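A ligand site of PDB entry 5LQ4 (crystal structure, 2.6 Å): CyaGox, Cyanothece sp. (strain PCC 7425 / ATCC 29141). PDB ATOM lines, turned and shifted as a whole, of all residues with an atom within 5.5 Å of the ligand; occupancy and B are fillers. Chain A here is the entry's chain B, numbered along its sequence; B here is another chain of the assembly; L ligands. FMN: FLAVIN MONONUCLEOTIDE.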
ATOM      1  N   ARG A 278       2.167 -17.926  -9.920  1.00  0.00           N
ATOM      2  CA  ARG A 278       1.853 -19.137 -10.674  1.00  0.00           C
ATOM      3  C   ARG A 278       3.064 -19.781 -11.350  1.00  0.00           C
ATOM      4  O   ARG A 278       3.806 -19.130 -12.078  1.00  0.00           O
ATOM      5  CB  ARG A 278       0.782 -18.831 -11.722  1.00  0.00           C
ATOM      6  CG  ARG A 278       0.269 -20.039 -12.499  1.00  0.00           C
ATOM      7  CD  ARG A 278      -0.067 -19.677 -13.939  1.00  0.00           C
ATOM      8  NE  ARG A 278       1.088 -19.120 -14.629  1.00  0.00           N
ATOM      9  CZ  ARG A 278       2.125 -19.825 -15.076  1.00  0.00           C
ATOM     10  NH1 ARG A 278       2.166 -21.152 -14.946  1.00  0.00           N
ATOM     11  NH2 ARG A 278       3.140 -19.194 -15.680  1.00  0.00           N
ATOM     12  N   ARG A 279       3.248 -21.065 -11.074  1.00  0.00           N
ATOM     13  CA  ARG A 279       4.314 -21.890 -11.585  1.00  0.00           C
ATOM     14  C   ARG A 279       3.725 -23.236 -12.015  1.00  0.00           C
ATOM     15  O   ARG A 279       2.700 -23.674 -11.486  1.00  0.00           O
ATOM     16  CB  ARG A 279       5.287 -22.044 -10.417  1.00  0.00           C
ATOM     17  CG  ARG A 279       6.612 -22.760 -10.659  1.00  0.00           C
ATOM     18  CD  ARG A 279       7.214 -23.172  -9.313  1.00  0.00           C
ATOM     19  NE  ARG A 279       8.653 -23.464  -9.391  1.00  0.00           N
ATOM     20  CZ  ARG A 279       9.213 -24.678  -9.455  1.00  0.00           C
ATOM     21  NH1 ARG A 279       8.496 -25.812  -9.505  1.00  0.00           N
ATOM     22  NH2 ARG A 279      10.546 -24.772  -9.502  1.00  0.00           N
ATOM     23  N   SER A 280       4.386 -23.905 -12.953  1.00  0.00           N
ATOM     24  CA  SER A 280       4.083 -25.307 -13.242  1.00  0.00           C
ATOM     25  C   SER A 280       4.959 -26.127 -12.305  1.00  0.00           C
ATOM     26  O   SER A 280       6.190 -25.995 -12.324  1.00  0.00           O
ATOM     27  CB  SER A 280       4.411 -25.662 -14.690  1.00  0.00           C
ATOM     28  OG  SER A 280       3.472 -25.091 -15.563  1.00  0.00           O
ATOM     29  N   ARG A 282       5.817 -29.964 -11.008  1.00  0.00           N
ATOM     30  CA  ARG A 282       5.762 -31.368 -11.388  1.00  0.00           C
ATOM     31  C   ARG A 282       6.286 -32.310 -10.316  1.00  0.00           C
ATOM     32  O   ARG A 282       5.995 -33.487 -10.367  1.00  0.00           O
ATOM     33  CB  ARG A 282       6.537 -31.584 -12.693  1.00  0.00           C
ATOM     34  CG  ARG A 282       5.949 -30.805 -13.857  1.00  0.00           C
ATOM     35  CD  ARG A 282       6.944 -30.632 -14.994  1.00  0.00           C
ATOM     36  NE  ARG A 282       6.472 -29.658 -15.990  1.00  0.00           N
ATOM     37  CZ  ARG A 282       6.720 -28.360 -16.044  1.00  0.00           C
ATOM     38  NH1 ARG A 282       7.490 -27.753 -15.145  1.00  0.00           N
ATOM     39  NH2 ARG A 282       6.188 -27.653 -17.044  1.00  0.00           N
ATOM     40  N   ALA A 380       4.848 -37.340 -20.347  1.00  0.00           N
ATOM     41  CA  ALA A 380       4.583 -36.020 -20.917  1.00  0.00           C
ATOM     42  C   ALA A 380       5.038 -34.851 -20.059  1.00  0.00           C
ATOM     43  O   ALA A 380       5.268 -33.757 -20.580  1.00  0.00           O
ATOM     44  CB  ALA A 380       3.102 -35.854 -21.228  1.00  0.00           C
ATOM     45  N   THR A 381       5.166 -35.065 -18.742  1.00  0.00           N
ATOM     46  CA  THR A 381       5.606 -34.019 -17.806  1.00  0.00           C
ATOM     47  C   THR A 381       7.059 -34.234 -17.356  1.00  0.00           C
ATOM     48  O   THR A 381       7.438 -33.774 -16.280  1.00  0.00           O
ATOM     49  CB  THR A 381       4.705 -33.946 -16.565  1.00  0.00           C
ATOM     50  OG1 THR A 381       4.570 -35.250 -16.019  1.00  0.00           O
ATOM     51  CG2 THR A 381       3.344 -33.376 -16.912  1.00  0.00           C
ATOM     52  N   GLY A 382       7.836 -34.966 -18.153  1.00  0.00           N
ATOM     53  CA  GLY A 382       9.267 -35.101 -17.931  1.00  0.00           C
ATOM     54  C   GLY A 382       9.747 -36.215 -17.008  1.00  0.00           C
ATOM     55  O   GLY A 382      10.935 -36.298 -16.750  1.00  0.00           O
ATOM     56  N   TYR A 420      -7.610 -24.473 -18.170  1.00  0.00           N
ATOM     57  CA  TYR A 420      -6.223 -24.616 -17.730  1.00  0.00           C
ATOM     58  C   TYR A 420      -5.745 -23.456 -16.868  1.00  0.00           C
ATOM     59  O   TYR A 420      -5.164 -23.682 -15.821  1.00  0.00           O
ATOM     60  CB  TYR A 420      -5.291 -24.719 -18.944  1.00  0.00           C
ATOM     61  CG  TYR A 420      -5.227 -26.073 -19.636  1.00  0.00           C
ATOM     62  CD1 TYR A 420      -6.068 -27.143 -19.281  1.00  0.00           C
ATOM     63  CD2 TYR A 420      -4.311 -26.277 -20.655  1.00  0.00           C
ATOM     64  CE1 TYR A 420      -5.991 -28.364 -19.933  1.00  0.00           C
ATOM     65  CE2 TYR A 420      -4.210 -27.494 -21.303  1.00  0.00           C
ATOM     66  CZ  TYR A 420      -5.051 -28.520 -20.947  1.00  0.00           C
ATOM     67  OH  TYR A 420      -4.942 -29.720 -21.618  1.00  0.00           O
ATOM     68  N   TYR A 424      -4.802 -23.445 -13.010  1.00  0.00           N
ATOM     69  CA  TYR A 424      -3.480 -22.957 -12.597  1.00  0.00           C
ATOM     70  C   TYR A 424      -3.559 -21.977 -11.440  1.00  0.00           C
ATOM     71  O   TYR A 424      -2.786 -22.074 -10.479  1.00  0.00           O
ATOM     72  CB  TYR A 424      -2.745 -22.293 -13.772  1.00  0.00           C
ATOM     73  CG  TYR A 424      -1.722 -23.156 -14.499  1.00  0.00           C
ATOM     74  CD1 TYR A 424      -0.511 -23.497 -13.888  1.00  0.00           C
ATOM     75  CD2 TYR A 424      -1.932 -23.579 -15.813  1.00  0.00           C
ATOM     76  CE1 TYR A 424       0.437 -24.269 -14.550  1.00  0.00           C
ATOM     77  CE2 TYR A 424      -0.995 -24.350 -16.483  1.00  0.00           C
ATOM     78  CZ  TYR A 424       0.188 -24.685 -15.855  1.00  0.00           C
ATOM     79  OH  TYR A 424       1.116 -25.442 -16.534  1.00  0.00           O
ATOM     80  N   SER A 435       0.123 -28.635 -13.448  1.00  0.00           N
ATOM     81  CA  SER A 435       0.733 -28.528 -14.764  1.00  0.00           C
ATOM     82  C   SER A 435      -0.241 -28.987 -15.832  1.00  0.00           C
ATOM     83  O   SER A 435      -0.847 -30.055 -15.713  1.00  0.00           O
ATOM     84  CB  SER A 435       2.022 -29.353 -14.884  1.00  0.00           C
ATOM     85  OG  SER A 435       2.706 -29.054 -16.096  1.00  0.00           O
ATOM     86  N   ALA A 436      -0.362 -28.168 -16.878  1.00  0.00           N
ATOM     87  CA  ALA A 436      -1.067 -28.566 -18.086  1.00  0.00           C
ATOM     88  C   ALA A 436      -0.266 -29.643 -18.803  1.00  0.00           C
ATOM     89  O   ALA A 436       0.937 -29.778 -18.597  1.00  0.00           O
ATOM     90  CB  ALA A 436      -1.285 -27.365 -19.001  1.00  0.00           C
ATOM     91  N   ILE A 437      -0.967 -30.440 -19.601  1.00  0.00           N
ATOM     92  CA  ILE A 437      -0.364 -31.506 -20.390  1.00  0.00           C
ATOM     93  C   ILE A 437      -0.829 -31.313 -21.828  1.00  0.00           C
ATOM     94  O   ILE A 437      -2.021 -31.136 -22.085  1.00  0.00           O
ATOM     95  CB  ILE A 437      -0.719 -32.918 -19.844  1.00  0.00           C
ATOM     96  CG1 ILE A 437      -0.235 -33.062 -18.392  1.00  0.00           C
ATOM     97  CG2 ILE A 437      -0.121 -34.016 -20.715  1.00  0.00           C
ATOM     98  CD1 ILE A 437      -0.699 -34.315 -17.686  1.00  0.00           C
ATOM     99  N   GLY A 438       0.113 -31.343 -22.759  1.00  0.00           N
ATOM    100  CA  GLY A 438      -0.150 -30.961 -24.143  1.00  0.00           C
ATOM    101  C   GLY A 438      -0.907 -31.992 -24.963  1.00  0.00           C
ATOM    102  O   GLY A 438      -1.716 -31.622 -25.814  1.00  0.00           O
ATOM    103  N   ALA A 439      -0.640 -33.261 -24.708  1.00  0.00           N
ATOM    104  CA  ALA A 439      -1.160 -34.352 -25.528  1.00  0.00           C
ATOM    105  C   ALA A 439      -1.866 -35.394 -24.676  1.00  0.00           C
ATOM    106  O   ALA A 439      -1.730 -35.407 -23.460  1.00  0.00           O
ATOM    107  CB  ALA A 439      -0.009 -34.994 -26.305  1.00  0.00           C
ATOM    108  N   PRO B 324       1.012 -19.134 -18.546  1.00  0.00           N
ATOM    109  CA  PRO B 324       1.738 -20.326 -18.968  1.00  0.00           C
ATOM    110  C   PRO B 324       1.676 -20.542 -20.475  1.00  0.00           C
ATOM    111  O   PRO B 324       0.794 -20.013 -21.118  1.00  0.00           O
ATOM    112  CB  PRO B 324       0.994 -21.461 -18.255  1.00  0.00           C
ATOM    113  CG  PRO B 324      -0.403 -20.980 -18.227  1.00  0.00           C
ATOM    114  CD  PRO B 324      -0.275 -19.500 -17.913  1.00  0.00           C
ATOM    115  N   SER B 325       2.629 -21.304 -21.002  1.00  0.00           N
ATOM    116  CA  SER B 325       2.736 -21.533 -22.430  1.00  0.00           C
ATOM    117  C   SER B 325       3.586 -22.776 -22.686  1.00  0.00           C
ATOM    118  O   SER B 325       4.766 -22.849 -22.302  1.00  0.00           O
ATOM    119  CB  SER B 325       3.342 -20.306 -23.134  1.00  0.00           C
ATOM    120  OG  SER B 325       3.162 -20.371 -24.545  1.00  0.00           O
ATOM    121  N   GLY B 326       2.936 -23.777 -23.283  1.00  0.00           N
ATOM    122  CA  GLY B 326       3.563 -24.897 -23.971  1.00  0.00           C
ATOM    123  C   GLY B 326       4.932 -24.654 -24.582  1.00  0.00           C
ATOM    124  O   GLY B 326       5.089 -23.825 -25.482  1.00  0.00           O
ATOM    125  N   GLY B 327       5.918 -25.349 -24.040  1.00  0.00           N
ATOM    126  CA  GLY B 327       7.309 -25.227 -24.463  1.00  0.00           C
ATOM    127  C   GLY B 327       8.006 -23.944 -24.070  1.00  0.00           C
ATOM    128  O   GLY B 327       9.125 -23.716 -24.514  1.00  0.00           O
ATOM    129  N   ALA B 328       7.379 -23.144 -23.200  1.00  0.00           N
ATOM    130  CA  ALA B 328       7.694 -21.725 -23.042  1.00  0.00           C
ATOM    131  C   ALA B 328       7.530 -21.093 -24.440  1.00  0.00           C
ATOM    132  O   ALA B 328       6.436 -21.216 -25.016  1.00  0.00           O
ATOM    133  CB  ALA B 328       9.079 -21.522 -22.437  1.00  0.00           C
ATOM    134  N   TYR B 330       6.471 -18.740 -26.208  1.00  0.00           N
ATOM    135  CA  TYR B 330       5.627 -17.545 -26.256  1.00  0.00           C
ATOM    136  C   TYR B 330       5.507 -16.926 -27.658  1.00  0.00           C
ATOM    137  O   TYR B 330       6.036 -15.841 -27.942  1.00  0.00           O
ATOM    138  CB  TYR B 330       6.122 -16.532 -25.239  1.00  0.00           C
ATOM    139  CG  TYR B 330       5.845 -16.983 -23.844  1.00  0.00           C
ATOM    140  CD1 TYR B 330       4.565 -16.866 -23.304  1.00  0.00           C
ATOM    141  CD2 TYR B 330       6.838 -17.534 -23.037  1.00  0.00           C
ATOM    142  CE1 TYR B 330       4.287 -17.267 -22.018  1.00  0.00           C
ATOM    143  CE2 TYR B 330       6.577 -17.943 -21.739  1.00  0.00           C
ATOM    144  CZ  TYR B 330       5.293 -17.803 -21.242  1.00  0.00           C
ATOM    145  OH  TYR B 330       5.016 -18.198 -19.970  1.00  0.00           O
ATOM    146  N   LEU B 409      -1.920 -26.439 -29.385  1.00  0.00           N
ATOM    147  CA  LEU B 409      -1.312 -25.672 -28.312  1.00  0.00           C
ATOM    148  C   LEU B 409      -1.639 -24.181 -28.424  1.00  0.00           C
ATOM    149  O   LEU B 409      -2.025 -23.557 -27.441  1.00  0.00           O
ATOM    150  CB  LEU B 409       0.192 -25.845 -28.301  1.00  0.00           C
ATOM    151  CG  LEU B 409       0.705 -27.145 -27.705  1.00  0.00           C
ATOM    152  CD1 LEU B 409       2.184 -27.242 -28.008  1.00  0.00           C
ATOM    153  CD2 LEU B 409       0.425 -27.207 -26.204  1.00  0.00           C
ATOM    154  N   LYS B 412      -5.167 -23.365 -27.310  1.00  0.00           N
ATOM    155  CA  LYS B 412      -5.207 -23.415 -25.848  1.00  0.00           C
ATOM    156  C   LYS B 412      -4.524 -22.218 -25.200  1.00  0.00           C
ATOM    157  O   LYS B 412      -4.940 -21.780 -24.134  1.00  0.00           O
ATOM    158  CB  LYS B 412      -4.570 -24.690 -25.321  1.00  0.00           C
ATOM    159  CG  LYS B 412      -5.365 -25.941 -25.629  1.00  0.00           C
ATOM    160  CD  LYS B 412      -4.594 -27.164 -25.221  1.00  0.00           C
ATOM    161  CE  LYS B 412      -5.280 -28.396 -25.754  1.00  0.00           C
ATOM    162  NZ  LYS B 412      -4.528 -29.589 -25.304  1.00  0.00           N
ATOM    163  N   HIS B 413      -3.457 -21.714 -25.838  1.00  0.00           N
ATOM    164  CA  HIS B 413      -2.810 -20.461 -25.398  1.00  0.00           C
ATOM    165  C   HIS B 413      -3.736 -19.251 -25.527  1.00  0.00           C
ATOM    166  O   HIS B 413      -3.728 -18.374 -24.669  1.00  0.00           O
ATOM    167  CB  HIS B 413      -1.493 -20.199 -26.133  1.00  0.00           C
ATOM    168  CG  HIS B 413      -0.471 -21.263 -25.949  1.00  0.00           C
ATOM    169  ND1 HIS B 413       0.544 -21.486 -26.849  1.00  0.00           N
ATOM    170  CD2 HIS B 413      -0.307 -22.183 -24.974  1.00  0.00           C
ATOM    171  CE1 HIS B 413       1.293 -22.490 -26.444  1.00  0.00           C
ATOM    172  NE2 HIS B 413       0.798 -22.923 -25.296  1.00  0.00           N
ATOM    173  N   VAL B 416      -6.008 -19.572 -22.604  1.00  0.00           N
ATOM    174  CA  VAL B 416      -5.232 -19.207 -21.414  1.00  0.00           C
ATOM    175  C   VAL B 416      -5.165 -17.678 -21.273  1.00  0.00           C
ATOM    176  O   VAL B 416      -5.316 -17.141 -20.164  1.00  0.00           O
ATOM    177  CB  VAL B 416      -3.812 -19.809 -21.460  1.00  0.00           C
ATOM    178  CG1 VAL B 416      -2.865 -19.106 -20.476  1.00  0.00           C
ATOM    179  CG2 VAL B 416      -3.866 -21.295 -21.162  1.00  0.00           C
HETATM  180  N1  FMN L   1       4.297 -28.832 -19.254  1.00  0.00           N
HETATM  181  C2  FMN L   1       4.772 -30.103 -19.398  1.00  0.00           C
HETATM  182  O2  FMN L   1       5.698 -30.497 -18.659  1.00  0.00           O
HETATM  183  N3  FMN L   1       4.276 -30.966 -20.315  1.00  0.00           N
HETATM  184  C4  FMN L   1       3.283 -30.618 -21.137  1.00  0.00           C
HETATM  185  O4  FMN L   1       2.863 -31.450 -21.961  1.00  0.00           O
HETATM  186  C4A FMN L   1       2.717 -29.242 -21.053  1.00  0.00           C
HETATM  187  N5  FMN L   1       1.712 -28.817 -21.851  1.00  0.00           N
HETATM  188  C5A FMN L   1       1.199 -27.561 -21.753  1.00  0.00           C
HETATM  189  C6  FMN L   1       0.159 -27.182 -22.602  1.00  0.00           C
HETATM  190  C7  FMN L   1      -0.399 -25.910 -22.538  1.00  0.00           C
HETATM  191  C7M FMN L   1      -1.518 -25.531 -23.474  1.00  0.00           C
HETATM  192  C8  FMN L   1       0.120 -24.930 -21.534  1.00  0.00           C
HETATM  193  C8M FMN L   1      -0.438 -23.538 -21.436  1.00  0.00           C
HETATM  194  C9  FMN L   1       1.162 -25.304 -20.698  1.00  0.00           C
HETATM  195  C9A FMN L   1       1.735 -26.593 -20.761  1.00  0.00           C
HETATM  196  N10 FMN L   1       2.787 -27.016 -19.907  1.00  0.00           N
HETATM  197  C10 FMN L   1       3.290 -28.340 -20.033  1.00  0.00           C
HETATM  198  C1' FMN L   1       3.377 -26.120 -18.911  1.00  0.00           C
HETATM  199  C2' FMN L   1       4.434 -25.296 -19.641  1.00  0.00           C
HETATM  200  O2' FMN L   1       5.518 -26.181 -19.992  1.00  0.00           O
HETATM  201  C3' FMN L   1       4.906 -24.134 -18.770  1.00  0.00           C
HETATM  202  O3' FMN L   1       3.866 -23.136 -18.769  1.00  0.00           O
HETATM  203  C4' FMN L   1       6.231 -23.517 -19.214  1.00  0.00           C
HETATM  204  O4' FMN L   1       7.140 -24.509 -19.731  1.00  0.00           O
HETATM  205  C5' FMN L   1       6.982 -22.907 -18.047  1.00  0.00           C
HETATM  206  O5' FMN L   1       6.186 -21.915 -17.419  1.00  0.00           O
HETATM  207  P   FMN L   1       5.644 -22.018 -15.899  1.00  0.00           P
HETATM  208  O1P FMN L   1       5.543 -20.558 -15.526  1.00  0.00           O
HETATM  209  O2P FMN L   1       4.306 -22.701 -16.011  1.00  0.00           O
HETATM  210  O3P FMN L   1       6.655 -22.819 -15.110  1.00  0.00           O
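The backbone NH of Gly 438 lies within hydrogen-bond range of an oxygen (O4) of the ligand (2.9 Å).
OG of Ser 280 sits at hydrogen-bond distance from O2P of the ligand (2.6 Å).
NE of Arg 282 sits at hydrogen-bond distance from O2 of the ligand (2.9 Å).
N of Ser 280 lies close to O2P of the ligand, at 3.3 Å.
O1P of the ligand lies within salt-bridge range of NH2 of Arg 278, 2.8 Å away.
A nitrogen (N3) of the ligand sits at hydrogen-bond distance from the backbone carbonyl oxygen of Ala 380 (3.0 Å).
N of Ser 325 of chain B lies within hydrogen-bond range of O3' of the ligand.
N of Ala 436 lies within hydrogen-bond range of OH of Tyr 424 (3.1 Å).
A ring nitrogen (ND1) of His 413 of chain B lies close to the backbone carbonyl oxygen of Leu 409 of chain B (3.4 Å).
The side-chain hydroxyl of Ser 280 sits at hydrogen-bond distance from the side-chain hydroxyl of Tyr 424, 2.6 Å away.
The backbone carbonyl oxygen (O) of Ala 328 of chain B lies within hydrogen-bond range of the side-chain hydroxyl (OG) of Ser 325 of chain B, at 3.4 Å.
The backbone carbonyl oxygen (O) of Ile 437 lies within hydrogen-bond range of the side-chain hydroxyl (OH) of Tyr 420 (3.3 Å).
The backbone NH (N) of Gly 326 of chain B is in hydrogen-bond range of a ring nitrogen (NE2) of His 413 of chain B (3.1 Å).
The backbone carbonyl oxygen (O) of Ala 436 lies close to a nitrogen (N5) of the ligand (3.5 Å).
Thr 381 touches the ligand (CA to O2, 3.6 Å).
Tyr 420 touches the ligand.
OH of Tyr 424 touches C1' of the ligand, at 3.3 Å.
Ser 435 touches the ligand.
Ile 437 touches the ligand (C to N5, 3.6 Å).
Pro 324 of chain B touches the ligand (CB to O3', 3.4 Å).
Gly 326 of chain B touches the ligand (N to C9, 3.5 Å).
Ala 328 of chain B touches the ligand.
Leu 409 of chain B touches the ligand.
Lys 412 of chain B touches the ligand.
CD2 of His 413 of chain B touches C8M of the ligand (3.8 Å).
Of the 24 residues printed, 18 come within 4 Å of the ligand.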
